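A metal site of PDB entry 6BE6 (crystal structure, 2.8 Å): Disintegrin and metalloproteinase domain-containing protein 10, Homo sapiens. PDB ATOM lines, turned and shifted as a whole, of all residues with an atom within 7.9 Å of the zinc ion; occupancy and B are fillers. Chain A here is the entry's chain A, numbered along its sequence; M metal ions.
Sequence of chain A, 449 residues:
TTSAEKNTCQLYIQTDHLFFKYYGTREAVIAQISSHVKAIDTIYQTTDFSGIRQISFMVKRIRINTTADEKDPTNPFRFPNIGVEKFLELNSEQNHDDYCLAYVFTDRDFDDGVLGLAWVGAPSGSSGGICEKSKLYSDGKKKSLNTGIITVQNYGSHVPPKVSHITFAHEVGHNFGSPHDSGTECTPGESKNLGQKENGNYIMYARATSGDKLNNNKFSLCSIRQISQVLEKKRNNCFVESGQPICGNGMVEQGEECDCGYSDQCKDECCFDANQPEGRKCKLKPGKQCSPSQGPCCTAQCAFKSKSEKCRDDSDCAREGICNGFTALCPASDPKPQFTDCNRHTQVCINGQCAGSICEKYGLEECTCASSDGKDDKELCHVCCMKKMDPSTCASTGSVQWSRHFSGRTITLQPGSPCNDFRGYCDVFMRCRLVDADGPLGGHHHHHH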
ATOM      1  N   GLY A 116     -11.476   4.205 -31.486  1.00  0.00           N
ATOM      2  CA  GLY A 116     -12.466   5.273 -31.491  1.00  0.00           C
ATOM      3  C   GLY A 116     -11.804   6.611 -31.267  1.00  0.00           C
ATOM      4  O   GLY A 116     -10.610   6.693 -30.953  1.00  0.00           O
ATOM      5  N   LEU A 117     -12.594   7.670 -31.445  1.00  0.00           N
ATOM      6  CA  LEU A 117     -12.098   9.027 -31.250  1.00  0.00           C
ATOM      7  C   LEU A 117     -13.285   9.931 -30.960  1.00  0.00           C
ATOM      8  O   LEU A 117     -14.290   9.885 -31.673  1.00  0.00           O
ATOM      9  CB  LEU A 117     -11.334   9.518 -32.481  1.00  0.00           C
ATOM     10  CG  LEU A 117     -10.401  10.713 -32.271  1.00  0.00           C
ATOM     11  CD1 LEU A 117      -9.184  10.305 -31.467  1.00  0.00           C
ATOM     12  CD2 LEU A 117      -9.993  11.315 -33.603  1.00  0.00           C
ATOM     13  N   ALA A 118     -13.161  10.753 -29.923  1.00  0.00           N
ATOM     14  CA  ALA A 118     -14.238  11.658 -29.540  1.00  0.00           C
ATOM     15  C   ALA A 118     -13.658  12.878 -28.848  1.00  0.00           C
ATOM     16  O   ALA A 118     -12.532  12.856 -28.340  1.00  0.00           O
ATOM     17  CB  ALA A 118     -15.256  10.966 -28.632  1.00  0.00           C
ATOM     18  N   VAL A 120     -13.437  15.660 -25.865  1.00  0.00           N
ATOM     19  CA  VAL A 120     -13.506  15.584 -24.403  1.00  0.00           C
ATOM     20  C   VAL A 120     -14.323  16.754 -23.887  1.00  0.00           C
ATOM     21  O   VAL A 120     -14.070  17.914 -24.245  1.00  0.00           O
ATOM     22  CB  VAL A 120     -12.096  15.573 -23.788  1.00  0.00           C
ATOM     23  CG1 VAL A 120     -12.185  15.634 -22.274  1.00  0.00           C
ATOM     24  CG2 VAL A 120     -11.340  14.337 -24.232  1.00  0.00           C
ATOM     25  N   THR A 167     -15.943  -0.052 -25.767  1.00  0.00           N
ATOM     26  CA  THR A 167     -15.294   1.022 -26.516  1.00  0.00           C
ATOM     27  C   THR A 167     -16.264   2.142 -26.822  1.00  0.00           C
ATOM     28  O   THR A 167     -15.886   3.325 -26.792  1.00  0.00           O
ATOM     29  CB  THR A 167     -14.692   0.462 -27.805  1.00  0.00           C
ATOM     30  OG1 THR A 167     -13.956  -0.730 -27.522  1.00  0.00           O
ATOM     31  CG2 THR A 167     -13.753   1.470 -28.440  1.00  0.00           C
ATOM     32  N   HIS A 170     -16.472   3.978 -23.756  1.00  0.00           N
ATOM     33  CA  HIS A 170     -15.205   4.669 -23.527  1.00  0.00           C
ATOM     34  C   HIS A 170     -15.205   6.052 -24.170  1.00  0.00           C
ATOM     35  O   HIS A 170     -14.917   7.054 -23.507  1.00  0.00           O
ATOM     36  CB  HIS A 170     -14.048   3.822 -24.066  1.00  0.00           C
ATOM     37  CG  HIS A 170     -12.702   4.434 -23.856  1.00  0.00           C
ATOM     38  ND1 HIS A 170     -11.935   4.171 -22.736  1.00  0.00           N
ATOM     39  CD2 HIS A 170     -11.978   5.280 -24.620  1.00  0.00           C
ATOM     40  CE1 HIS A 170     -10.795   4.840 -22.825  1.00  0.00           C
ATOM     41  NE2 HIS A 170     -10.793   5.520 -23.950  1.00  0.00           N
ATOM     42  N   GLU A 171     -15.537   6.123 -25.456  1.00  0.00           N
ATOM     43  CA  GLU A 171     -15.532   7.411 -26.155  1.00  0.00           C
ATOM     44  C   GLU A 171     -16.631   8.325 -25.619  1.00  0.00           C
ATOM     45  O   GLU A 171     -16.423   9.531 -25.479  1.00  0.00           O
ATOM     46  CB  GLU A 171     -15.688   7.198 -27.661  1.00  0.00           C
ATOM     47  CG  GLU A 171     -14.561   6.398 -28.285  1.00  0.00           C
ATOM     48  CD  GLU A 171     -13.203   7.063 -28.108  1.00  0.00           C
ATOM     49  OE1 GLU A 171     -13.138   8.310 -28.088  1.00  0.00           O
ATOM     50  OE2 GLU A 171     -12.192   6.323 -28.004  1.00  0.00           O
ATOM     51  N   GLY A 173     -17.534   8.337 -22.665  1.00  0.00           N
ATOM     52  CA  GLY A 173     -16.951   8.842 -21.427  1.00  0.00           C
ATOM     53  C   GLY A 173     -16.207  10.145 -21.629  1.00  0.00           C
ATOM     54  O   GLY A 173     -16.341  11.079 -20.822  1.00  0.00           O
ATOM     55  N   HIS A 174     -15.415  10.229 -22.700  1.00  0.00           N
ATOM     56  CA  HIS A 174     -14.749  11.493 -23.014  1.00  0.00           C
ATOM     57  C   HIS A 174     -15.768  12.587 -23.307  1.00  0.00           C
ATOM     58  O   HIS A 174     -15.597  13.734 -22.878  1.00  0.00           O
ATOM     59  CB  HIS A 174     -13.817  11.313 -24.219  1.00  0.00           C
ATOM     60  CG  HIS A 174     -12.705  10.336 -23.986  1.00  0.00           C
ATOM     61  ND1 HIS A 174     -11.717  10.549 -23.039  1.00  0.00           N
ATOM     62  CD2 HIS A 174     -12.419   9.155 -24.572  1.00  0.00           C
ATOM     63  CE1 HIS A 174     -10.872   9.536 -23.058  1.00  0.00           C
ATOM     64  NE2 HIS A 174     -11.271   8.672 -23.974  1.00  0.00           N
ATOM     65  N   SER A 178     -14.703  12.855 -19.147  1.00  0.00           N
ATOM     66  CA  SER A 178     -13.798  11.996 -18.401  1.00  0.00           C
ATOM     67  C   SER A 178     -12.504  11.795 -19.170  1.00  0.00           C
ATOM     68  O   SER A 178     -12.551  11.329 -20.319  1.00  0.00           O
ATOM     69  CB  SER A 178     -14.441  10.644 -18.107  1.00  0.00           C
ATOM     70  OG  SER A 178     -13.481   9.748 -17.579  1.00  0.00           O
ATOM     71  N   PRO A 179     -11.353  12.118 -18.595  1.00  0.00           N
ATOM     72  CA  PRO A 179     -10.086  11.749 -19.235  1.00  0.00           C
ATOM     73  C   PRO A 179      -9.780  10.277 -19.027  1.00  0.00           C
ATOM     74  O   PRO A 179     -10.624   9.533 -18.514  1.00  0.00           O
ATOM     75  CB  PRO A 179      -9.069  12.649 -18.521  1.00  0.00           C
ATOM     76  CG  PRO A 179      -9.664  12.856 -17.163  1.00  0.00           C
ATOM     77  CD  PRO A 179     -11.151  12.901 -17.360  1.00  0.00           C
ATOM     78  N   HIS A 180      -8.587   9.855 -19.412  1.00  0.00           N
ATOM     79  CA  HIS A 180      -8.177   8.481 -19.175  1.00  0.00           C
ATOM     80  C   HIS A 180      -7.869   8.259 -17.696  1.00  0.00           C
ATOM     81  O   HIS A 180      -7.427   9.162 -16.996  1.00  0.00           O
ATOM     82  CB  HIS A 180      -6.962   8.123 -20.024  1.00  0.00           C
ATOM     83  CG  HIS A 180      -7.265   7.981 -21.483  1.00  0.00           C
ATOM     84  ND1 HIS A 180      -6.358   8.302 -22.467  1.00  0.00           N
ATOM     85  CD2 HIS A 180      -8.375   7.538 -22.118  1.00  0.00           C
ATOM     86  CE1 HIS A 180      -6.894   8.067 -23.656  1.00  0.00           C
ATOM     87  NE2 HIS A 180      -8.125   7.605 -23.469  1.00  0.00           N
ATOM     88  N   ASP A 181      -8.118   7.035 -17.236  1.00  0.00           N
ATOM     89  CA  ASP A 181      -7.818   6.685 -15.860  1.00  0.00           C
ATOM     90  C   ASP A 181      -6.311   6.717 -15.630  1.00  0.00           C
ATOM     91  O   ASP A 181      -5.521   6.294 -16.478  1.00  0.00           O
ATOM     92  CB  ASP A 181      -8.363   5.300 -15.521  1.00  0.00           C
ATOM     93  CG  ASP A 181      -9.875   5.293 -15.409  1.00  0.00           C
ATOM     94  OD1 ASP A 181     -10.460   6.354 -15.127  1.00  0.00           O
ATOM     95  OD2 ASP A 181     -10.472   4.206 -15.599  1.00  0.00           O
ATOM     96  N   ILE A 203     -13.424   1.340 -17.330  1.00  0.00           N
ATOM     97  CA  ILE A 203     -13.854   1.659 -18.696  1.00  0.00           C
ATOM     98  C   ILE A 203     -12.884   2.628 -19.353  1.00  0.00           C
ATOM     99  O   ILE A 203     -12.440   2.429 -20.484  1.00  0.00           O
ATOM    100  CB  ILE A 203     -15.287   2.212 -18.694  1.00  0.00           C
ATOM    101  CG1 ILE A 203     -16.287   1.100 -18.345  1.00  0.00           C
ATOM    102  CG2 ILE A 203     -15.617   2.842 -20.032  1.00  0.00           C
ATOM    103  CD1 ILE A 203     -17.728   1.540 -18.444  1.00  0.00           C
ATOM    104  N   MET A 204     -12.543   3.716 -18.647  1.00  0.00           N
ATOM    105  CA  MET A 204     -11.688   4.760 -19.188  1.00  0.00           C
ATOM    106  C   MET A 204     -10.207   4.416 -19.089  1.00  0.00           C
ATOM    107  O   MET A 204      -9.366   5.310 -18.936  1.00  0.00           O
ATOM    108  CB  MET A 204     -11.979   6.089 -18.493  1.00  0.00           C
ATOM    109  CG  MET A 204     -13.443   6.506 -18.596  1.00  0.00           C
ATOM    110  SD  MET A 204     -14.049   6.517 -20.297  1.00  0.00           S
ATOM    111  CE  MET A 204     -13.073   7.852 -20.990  1.00  0.00           C
ATOM    112  N   TYR A 205      -9.857   3.133 -19.187  1.00  0.00           N
ATOM    113  CA  TYR A 205      -8.460   2.748 -19.286  1.00  0.00           C
ATOM    114  C   TYR A 205      -7.898   3.149 -20.642  1.00  0.00           C
ATOM    115  O   TYR A 205      -8.533   2.953 -21.674  1.00  0.00           O
ATOM    116  CB  TYR A 205      -8.307   1.242 -19.059  1.00  0.00           C
ATOM    117  CG  TYR A 205      -6.875   0.774 -18.970  1.00  0.00           C
ATOM    118  CD1 TYR A 205      -6.014   1.291 -18.019  1.00  0.00           C
ATOM    119  CD2 TYR A 205      -6.387  -0.202 -19.833  1.00  0.00           C
ATOM    120  CE1 TYR A 205      -4.702   0.865 -17.940  1.00  0.00           C
ATOM    121  CE2 TYR A 205      -5.087  -0.635 -19.750  1.00  0.00           C
ATOM    122  CZ  TYR A 205      -4.250  -0.099 -18.801  1.00  0.00           C
ATOM    123  OH  TYR A 205      -2.944  -0.526 -18.713  1.00  0.00           O
ATOM    124  N   ALA A 206      -6.694   3.723 -20.631  1.00  0.00           N
ATOM    125  CA  ALA A 206      -6.132   4.312 -21.834  1.00  0.00           C
ATOM    126  C   ALA A 206      -5.625   3.285 -22.845  1.00  0.00           C
ATOM    127  O   ALA A 206      -5.369   3.657 -23.992  1.00  0.00           O
ATOM    128  CB  ALA A 206      -4.988   5.269 -21.472  1.00  0.00           C
ATOM    129  N   ARG A 207      -5.504   2.014 -22.457  1.00  0.00           N
ATOM    130  CA  ARG A 207      -4.914   1.041 -23.363  1.00  0.00           C
ATOM    131  C   ARG A 207      -5.904  -0.058 -23.752  1.00  0.00           C
ATOM    132  O   ARG A 207      -7.092   0.211 -23.915  1.00  0.00           O
ATOM    133  CB  ARG A 207      -3.662   0.429 -22.728  1.00  0.00           C
ATOM    134  CG  ARG A 207      -2.648   1.476 -22.283  1.00  0.00           C
ATOM    135  CD  ARG A 207      -1.386   0.847 -21.702  1.00  0.00           C
ATOM    136  NE  ARG A 207      -0.484   1.851 -21.155  1.00  0.00           N
ATOM    137  CZ  ARG A 207       0.688   1.570 -20.577  1.00  0.00           C
ATOM    138  NH1 ARG A 207       1.094   0.319 -20.471  1.00  0.00           N
ATOM    139  NH2 ARG A 207       1.447   2.549 -20.109  1.00  0.00           N
HETATM  140 ZN    ZN M   1      -9.875   7.320 -24.649  1.00  0.00          ZN
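O of Ile 203 sits at hydrogen-bond distance from ND1 of His 170 (2.9 Å). O of Ser 178 is in hydrogen-bond range of ND1 of His 174 (2.9 Å).
Within 4 Å of the zinc ion: His 170, His 174 and His 180.
The zinc ion is bound by NE2 of His 174, NE2 of His 180 and NE2 of His 170.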
